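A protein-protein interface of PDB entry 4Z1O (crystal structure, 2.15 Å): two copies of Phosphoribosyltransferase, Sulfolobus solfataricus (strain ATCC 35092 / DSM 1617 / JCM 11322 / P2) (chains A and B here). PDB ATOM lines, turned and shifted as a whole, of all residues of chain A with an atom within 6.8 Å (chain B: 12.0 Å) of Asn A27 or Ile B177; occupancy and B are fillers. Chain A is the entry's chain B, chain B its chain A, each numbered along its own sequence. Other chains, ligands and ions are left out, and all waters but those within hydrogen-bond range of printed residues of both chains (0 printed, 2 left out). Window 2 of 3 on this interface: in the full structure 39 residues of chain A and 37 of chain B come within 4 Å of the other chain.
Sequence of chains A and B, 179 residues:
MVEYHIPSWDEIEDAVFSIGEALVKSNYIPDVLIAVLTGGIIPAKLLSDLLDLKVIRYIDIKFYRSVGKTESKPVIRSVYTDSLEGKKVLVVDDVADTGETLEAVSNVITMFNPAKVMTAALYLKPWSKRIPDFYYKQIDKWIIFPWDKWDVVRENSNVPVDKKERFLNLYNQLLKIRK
Of chain B, only Leu B170 (3.7 Å), Gln B173 (3.8 Å), Leu B174 (3.9 Å) and Ile B177 (3.6 Å) come within 4 Å of Val A24. Ser A26 touches none of the printed residues of chain B. Of chain B, only Ile B177 (3.7 Å) comes within 4 Å of Asn A27. Ile A29 touches two residues of chain B. Of the printed residues of chain B, Lys A88 touches Arg B178 (3.2 Å). Of the printed residues of chain A, Leu B170 touches Val A24. Lys B176 touches none of the printed residues of chain A. Ile B177 touches two residues of chain A. Of the printed residues of chain A, Arg B178 touches Ile A29 and Lys A88. The nearest residue of chain A that does not touch Ile B177 is Ile A29 (4.1 Å). The nearest printed residue of chain A that does not touch Leu B170 is Ala A22 (5.9 Å).
The backbone carbonyl oxygen (O) of Ile A29 lies within hydrogen-bond range of the guanidinium group (NH1) of Arg B178, at 2.7 Å. NZ of Lys A88 sits close to NH1 of Arg B178 (3.2 Å).
Of the 13 printed residues of chain B, 5 touch a printed residue of chain A. Printed residues of chain B that touch a printed residue of chain A: Leu B170, Gln B173, Leu B174, Ile B177 and Arg B178. Hydrophobic or aromatic side chains of chain B within 4 Å of the printed part of chain A: Leu B170, Leu B174 and Ile B177. Of the 9 printed residues of chain A, 4 touch a printed residue of chain B. Among the printed residues, no Asp or Glu carboxylate lies within 4 Å of a Lys or Arg side-chain nitrogen of the other chain.
The backbone carbonyl oxygen of Ile A29 lies within hydrogen-bond range of the side-chain amino group of Lys A88, at 3.2 Å. The side-chain amide nitrogen (NE2) of Gln B173 sits at hydrogen-bond distance from the backbone carbonyl oxygen (O) of Asn B169 (3.1 Å).
Among the printed residues, merely in contact across the chains: Ile A29 with Leu B174 (3.4 Å), Val A24 with Ile B177 (3.6 Å), Val A24 with Leu B170 (3.7 Å), Asn A27 with Ile B177 (3.7 Å), Val A24 with Gln B173 (3.8 Å) and Val A24 with Leu B174 (3.9 Å).
No position is printed for both chains. Of the 8 pairs that touch across the chains among the printed residues, none has its exchanged pair printed and touching as well.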
ATOM      1  N   ALA A  22      12.785  -1.383 -24.156  1.00  0.00           N
ATOM      2  CA  ALA A  22      13.704  -2.513 -24.107  1.00  0.00           C
ATOM      3  C   ALA A  22      14.806  -2.282 -23.085  1.00  0.00           C
ATOM      4  O   ALA A  22      15.245  -3.221 -22.431  1.00  0.00           O
ATOM      5  CB  ALA A  22      14.307  -2.776 -25.474  1.00  0.00           C
ATOM      6  N   LEU A  23      15.260  -1.041 -22.956  1.00  0.00           N
ATOM      7  CA  LEU A  23      16.288  -0.718 -21.967  1.00  0.00           C
ATOM      8  C   LEU A  23      15.799  -0.956 -20.530  1.00  0.00           C
ATOM      9  O   LEU A  23      16.542  -1.468 -19.678  1.00  0.00           O
ATOM     10  CB  LEU A  23      16.736   0.732 -22.123  1.00  0.00           C
ATOM     11  CG  LEU A  23      17.690   1.016 -23.299  1.00  0.00           C
ATOM     12  CD1 LEU A  23      17.708   2.496 -23.614  1.00  0.00           C
ATOM     13  CD2 LEU A  23      19.101   0.505 -23.007  1.00  0.00           C
ATOM     14  N   VAL A  24      14.553  -0.570 -20.266  1.00  0.00           N
ATOM     15  CA  VAL A  24      13.971  -0.717 -18.932  1.00  0.00           C
ATOM     16  C   VAL A  24      13.683  -2.190 -18.674  1.00  0.00           C
ATOM     17  O   VAL A  24      13.960  -2.698 -17.599  1.00  0.00           O
ATOM     18  CB  VAL A  24      12.682   0.126 -18.757  1.00  0.00           C
ATOM     19  CG1 VAL A  24      11.957  -0.234 -17.457  1.00  0.00           C
ATOM     20  CG2 VAL A  24      13.017   1.590 -18.768  1.00  0.00           C
ATOM     21  N   LYS A  25      13.163  -2.871 -19.685  1.00  0.00           N
ATOM     22  CA  LYS A  25      12.911  -4.308 -19.632  1.00  0.00           C
ATOM     23  C   LYS A  25      14.180  -5.123 -19.345  1.00  0.00           C
ATOM     24  O   LYS A  25      14.111  -6.163 -18.690  1.00  0.00           O
ATOM     25  CB  LYS A  25      12.254  -4.767 -20.950  1.00  0.00           C
ATOM     26  CG  LYS A  25      12.498  -6.230 -21.345  1.00  0.00           C
ATOM     27  CD  LYS A  25      11.552  -6.672 -22.462  1.00  0.00           C
ATOM     28  CE  LYS A  25      12.212  -7.669 -23.433  1.00  0.00           C
ATOM     29  NZ  LYS A  25      12.734  -7.031 -24.686  1.00  0.00           N
ATOM     30  N   SER A  26      15.328  -4.639 -19.813  1.00  0.00           N
ATOM     31  CA  SER A  26      16.600  -5.328 -19.627  1.00  0.00           C
ATOM     32  C   SER A  26      17.315  -4.857 -18.371  1.00  0.00           C
ATOM     33  O   SER A  26      18.380  -5.369 -18.032  1.00  0.00           O
ATOM     34  CB  SER A  26      17.526  -5.110 -20.830  1.00  0.00           C
ATOM     35  OG  SER A  26      16.913  -5.500 -22.047  1.00  0.00           O
ATOM     36  N   ASN A  27      16.735  -3.859 -17.711  1.00  0.00           N
ATOM     37  CA  ASN A  27      17.371  -3.179 -16.576  1.00  0.00           C
ATOM     38  C   ASN A  27      18.767  -2.689 -16.949  1.00  0.00           C
ATOM     39  O   ASN A  27      19.738  -2.935 -16.235  1.00  0.00           O
ATOM     40  CB  ASN A  27      17.431  -4.099 -15.346  1.00  0.00           C
ATOM     41  CG  ASN A  27      17.713  -3.338 -14.047  1.00  0.00           C
ATOM     42  OD1 ASN A  27      17.594  -2.109 -13.988  1.00  0.00           O
ATOM     43  ND2 ASN A  27      18.078  -4.074 -13.000  1.00  0.00           N
ATOM     44  N   TYR A  28      18.865  -2.024 -18.098  1.00  0.00           N
ATOM     45  CA  TYR A  28      20.099  -1.361 -18.471  1.00  0.00           C
ATOM     46  C   TYR A  28      19.811   0.111 -18.662  1.00  0.00           C
ATOM     47  O   TYR A  28      19.400   0.542 -19.739  1.00  0.00           O
ATOM     48  CB  TYR A  28      20.714  -1.959 -19.739  1.00  0.00           C
ATOM     49  CG  TYR A  28      22.111  -1.428 -19.980  1.00  0.00           C
ATOM     50  CD1 TYR A  28      23.174  -1.873 -19.208  1.00  0.00           C
ATOM     51  CD2 TYR A  28      22.362  -0.450 -20.948  1.00  0.00           C
ATOM     52  CE1 TYR A  28      24.445  -1.398 -19.391  1.00  0.00           C
ATOM     53  CE2 TYR A  28      23.646   0.043 -21.141  1.00  0.00           C
ATOM     54  CZ  TYR A  28      24.688  -0.443 -20.355  1.00  0.00           C
ATOM     55  OH  TYR A  28      25.979   0.008 -20.519  1.00  0.00           O
ATOM     56  N   ILE A  29      19.980   0.868 -17.589  1.00  0.00           N
ATOM     57  CA  ILE A  29      19.835   2.300 -17.658  1.00  0.00           C
ATOM     58  C   ILE A  29      21.242   2.879 -17.697  1.00  0.00           C
ATOM     59  O   ILE A  29      22.001   2.734 -16.744  1.00  0.00           O
ATOM     60  CB  ILE A  29      19.029   2.856 -16.477  1.00  0.00           C
ATOM     61  CG1 ILE A  29      17.700   2.103 -16.347  1.00  0.00           C
ATOM     62  CG2 ILE A  29      18.747   4.343 -16.677  1.00  0.00           C
ATOM     63  CD1 ILE A  29      16.730   2.363 -17.504  1.00  0.00           C
ATOM     64  N   LYS A  88      28.249   2.818 -17.034  1.00  0.00           N
ATOM     65  CA  LYS A  88      27.428   2.094 -17.995  1.00  0.00           C
ATOM     66  C   LYS A  88      27.150   3.016 -19.172  1.00  0.00           C
ATOM     67  O   LYS A  88      26.493   4.035 -19.027  1.00  0.00           O
ATOM     68  CB  LYS A  88      26.125   1.609 -17.357  1.00  0.00           C
ATOM     69  CG  LYS A  88      26.374   0.611 -16.210  1.00  0.00           C
ATOM     70  CD  LYS A  88      25.077   0.072 -15.608  1.00  0.00           C
ATOM     71  CE  LYS A  88      24.249   1.199 -15.037  1.00  0.00           C
ATOM     72  NZ  LYS A  88      22.973   0.702 -14.462  1.00  0.00           N
ATOM     73  N   PHE B 167       4.081   6.924 -22.261  1.00  0.00           N
ATOM     74  CA  PHE B 167       5.194   7.406 -21.448  1.00  0.00           C
ATOM     75  C   PHE B 167       5.019   7.142 -19.956  1.00  0.00           C
ATOM     76  O   PHE B 167       5.961   6.701 -19.295  1.00  0.00           O
ATOM     77  CB  PHE B 167       5.422   8.897 -21.642  1.00  0.00           C
ATOM     78  CG  PHE B 167       6.398   9.476 -20.663  1.00  0.00           C
ATOM     79  CD1 PHE B 167       7.749   9.203 -20.773  1.00  0.00           C
ATOM     80  CD2 PHE B 167       5.962  10.282 -19.611  1.00  0.00           C
ATOM     81  CE1 PHE B 167       8.659   9.723 -19.847  1.00  0.00           C
ATOM     82  CE2 PHE B 167       6.861  10.805 -18.686  1.00  0.00           C
ATOM     83  CZ  PHE B 167       8.213  10.531 -18.808  1.00  0.00           C
ATOM     84  N   LEU B 168       3.840   7.451 -19.424  1.00  0.00           N
ATOM     85  CA  LEU B 168       3.578   7.210 -18.006  1.00  0.00           C
ATOM     86  C   LEU B 168       3.768   5.738 -17.709  1.00  0.00           C
ATOM     87  O   LEU B 168       4.307   5.367 -16.673  1.00  0.00           O
ATOM     88  CB  LEU B 168       2.177   7.669 -17.616  1.00  0.00           C
ATOM     89  CG  LEU B 168       2.003   9.192 -17.611  1.00  0.00           C
ATOM     90  CD1 LEU B 168       0.553   9.586 -17.370  1.00  0.00           C
ATOM     91  CD2 LEU B 168       2.917   9.857 -16.587  1.00  0.00           C
ATOM     92  N   ASN B 169       3.355   4.905 -18.655  1.00  0.00           N
ATOM     93  CA  ASN B 169       3.561   3.462 -18.575  1.00  0.00           C
ATOM     94  C   ASN B 169       5.023   3.041 -18.389  1.00  0.00           C
ATOM     95  O   ASN B 169       5.333   2.165 -17.585  1.00  0.00           O
ATOM     96  CB  ASN B 169       3.012   2.810 -19.837  1.00  0.00           C
ATOM     97  CG  ASN B 169       2.184   1.589 -19.546  1.00  0.00           C
ATOM     98  OD1 ASN B 169       0.988   1.689 -19.281  1.00  0.00           O
ATOM     99  ND2 ASN B 169       2.816   0.422 -19.594  1.00  0.00           N
ATOM    100  N   LEU B 170       5.915   3.655 -19.158  1.00  0.00           N
ATOM    101  CA  LEU B 170       7.335   3.319 -19.106  1.00  0.00           C
ATOM    102  C   LEU B 170       8.016   3.967 -17.908  1.00  0.00           C
ATOM    103  O   LEU B 170       8.863   3.358 -17.264  1.00  0.00           O
ATOM    104  CB  LEU B 170       8.041   3.757 -20.388  1.00  0.00           C
ATOM    105  CG  LEU B 170       9.537   3.445 -20.416  1.00  0.00           C
ATOM    106  CD1 LEU B 170       9.722   1.951 -20.395  1.00  0.00           C
ATOM    107  CD2 LEU B 170      10.220   4.052 -21.637  1.00  0.00           C
ATOM    108  N   TYR B 171       7.642   5.217 -17.639  1.00  0.00           N
ATOM    109  CA  TYR B 171       8.203   5.984 -16.535  1.00  0.00           C
ATOM    110  C   TYR B 171       7.931   5.269 -15.210  1.00  0.00           C
ATOM    111  O   TYR B 171       8.810   5.177 -14.370  1.00  0.00           O
ATOM    112  CB  TYR B 171       7.619   7.400 -16.517  1.00  0.00           C
ATOM    113  CG  TYR B 171       8.253   8.338 -15.505  1.00  0.00           C
ATOM    114  CD1 TYR B 171       9.555   8.132 -15.049  1.00  0.00           C
ATOM    115  CD2 TYR B 171       7.543   9.433 -14.998  1.00  0.00           C
ATOM    116  CE1 TYR B 171      10.134   8.981 -14.126  1.00  0.00           C
ATOM    117  CE2 TYR B 171       8.120  10.297 -14.070  1.00  0.00           C
ATOM    118  CZ  TYR B 171       9.418  10.066 -13.637  1.00  0.00           C
ATOM    119  OH  TYR B 171      10.003  10.908 -12.710  1.00  0.00           O
ATOM    120  N   ASN B 172       6.716   4.755 -15.043  1.00  0.00           N
ATOM    121  CA  ASN B 172       6.383   3.982 -13.856  1.00  0.00           C
ATOM    122  C   ASN B 172       7.355   2.844 -13.620  1.00  0.00           C
ATOM    123  O   ASN B 172       7.889   2.707 -12.527  1.00  0.00           O
ATOM    124  CB  ASN B 172       4.966   3.430 -13.947  1.00  0.00           C
ATOM    125  CG  ASN B 172       3.950   4.404 -13.440  1.00  0.00           C
ATOM    126  OD1 ASN B 172       4.155   5.044 -12.408  1.00  0.00           O
ATOM    127  ND2 ASN B 172       2.836   4.523 -14.150  1.00  0.00           N
ATOM    128  N   GLN B 173       7.603   2.032 -14.641  1.00  0.00           N
ATOM    129  CA  GLN B 173       8.541   0.927 -14.485  1.00  0.00           C
ATOM    130  C   GLN B 173       9.937   1.463 -14.233  1.00  0.00           C
ATOM    131  O   GLN B 173      10.700   0.888 -13.463  1.00  0.00           O
ATOM    132  CB  GLN B 173       8.536   0.028 -15.715  1.00  0.00           C
ATOM    133  CG  GLN B 173       7.158  -0.348 -16.183  1.00  0.00           C
ATOM    134  CD  GLN B 173       7.191  -1.093 -17.501  1.00  0.00           C
ATOM    135  OE1 GLN B 173       7.631  -2.244 -17.560  1.00  0.00           O
ATOM    136  NE2 GLN B 173       6.726  -0.440 -18.573  1.00  0.00           N
ATOM    137  N   LEU B 174      10.261   2.576 -14.887  1.00  0.00           N
ATOM    138  CA  LEU B 174      11.574   3.199 -14.733  1.00  0.00           C
ATOM    139  C   LEU B 174      11.803   3.603 -13.277  1.00  0.00           C
ATOM    140  O   LEU B 174      12.885   3.360 -12.714  1.00  0.00           O
ATOM    141  CB  LEU B 174      11.715   4.422 -15.654  1.00  0.00           C
ATOM    142  CG  LEU B 174      13.130   5.010 -15.691  1.00  0.00           C
ATOM    143  CD1 LEU B 174      14.138   3.901 -15.827  1.00  0.00           C
ATOM    144  CD2 LEU B 174      13.309   6.000 -16.827  1.00  0.00           C
ATOM    145  N   LEU B 175      10.782   4.209 -12.669  1.00  0.00           N
ATOM    146  CA  LEU B 175      10.889   4.678 -11.279  1.00  0.00           C
ATOM    147  C   LEU B 175      11.162   3.528 -10.309  1.00  0.00           C
ATOM    148  O   LEU B 175      11.852   3.709  -9.305  1.00  0.00           O
ATOM    149  CB  LEU B 175       9.621   5.424 -10.852  1.00  0.00           C
ATOM    150  CG  LEU B 175       9.363   6.836 -11.383  1.00  0.00           C
ATOM    151  CD1 LEU B 175       7.988   7.312 -10.928  1.00  0.00           C
ATOM    152  CD2 LEU B 175      10.444   7.795 -10.932  1.00  0.00           C
ATOM    153  N   LYS B 176      10.627   2.350 -10.624  1.00  0.00           N
ATOM    154  CA  LYS B 176      10.818   1.169  -9.780  1.00  0.00           C
ATOM    155  C   LYS B 176      12.250   0.682  -9.792  1.00  0.00           C
ATOM    156  O   LYS B 176      12.818   0.371  -8.745  1.00  0.00           O
ATOM    157  CB  LYS B 176       9.910   0.018 -10.217  1.00  0.00           C
ATOM    158  CG  LYS B 176       8.579  -0.069  -9.484  1.00  0.00           C
ATOM    159  CD  LYS B 176       7.591   0.977  -9.985  1.00  0.00           C
ATOM    160  CE  LYS B 176       6.162   0.562  -9.718  1.00  0.00           C
ATOM    161  NZ  LYS B 176       5.216   1.668  -9.998  1.00  0.00           N
ATOM    162  N   ILE B 177      12.837   0.609 -10.978  1.00  0.00           N
ATOM    163  CA  ILE B 177      14.076  -0.138 -11.125  1.00  0.00           C
ATOM    164  C   ILE B 177      15.318   0.693 -10.857  1.00  0.00           C
ATOM    165  O   ILE B 177      16.415   0.147 -10.755  1.00  0.00           O
ATOM    166  CB  ILE B 177      14.197  -0.761 -12.520  1.00  0.00           C
ATOM    167  CG1 ILE B 177      14.129   0.319 -13.604  1.00  0.00           C
ATOM    168  CG2 ILE B 177      13.114  -1.836 -12.717  1.00  0.00           C
ATOM    169  CD1 ILE B 177      14.557  -0.181 -14.974  1.00  0.00           C
ATOM    170  N   ARG B 178      15.168   2.005 -10.737  1.00  0.00           N
ATOM    171  CA  ARG B 178      16.297   2.790 -10.264  1.00  0.00           C
ATOM    172  C   ARG B 178      15.883   3.834  -9.229  1.00  0.00           C
ATOM    173  O   ARG B 178      15.332   4.885  -9.545  1.00  0.00           O
ATOM    174  CB  ARG B 178      17.035   3.442 -11.432  1.00  0.00           C
ATOM    175  CG  ARG B 178      18.535   3.488 -11.158  1.00  0.00           C
ATOM    176  CD  ARG B 178      19.395   3.713 -12.397  1.00  0.00           C
ATOM    177  NE  ARG B 178      20.808   3.773 -12.015  1.00  0.00           N
ATOM    178  CZ  ARG B 178      21.826   3.697 -12.868  1.00  0.00           C
ATOM    179  NH1 ARG B 178      21.594   3.568 -14.165  1.00  0.00           N
ATOM    180  NH2 ARG B 178      23.080   3.758 -12.434  1.00  0.00           N
ATOM    181  N   LYS B 179      16.172   3.510  -7.977  1.00  0.00           N
ATOM    182  CA  LYS B 179      15.792   4.336  -6.841  1.00  0.00           C
ATOM    183  C   LYS B 179      17.013   5.049  -6.263  1.00  0.00           C
ATOM    184  O   LYS B 179      18.134   4.532  -6.329  1.00  0.00           O
ATOM    185  CB  LYS B 179      15.122   3.475  -5.768  1.00  0.00           C
ATOM    186  CG  LYS B 179      13.989   2.584  -6.277  1.00  0.00           C
ATOM    187  CD  LYS B 179      13.711   1.476  -5.284  1.00  0.00           C
ATOM    188  CE  LYS B 179      12.318   0.905  -5.397  1.00  0.00           C
ATOM    189  NZ  LYS B 179      12.158  -0.257  -4.470  1.00  0.00           N
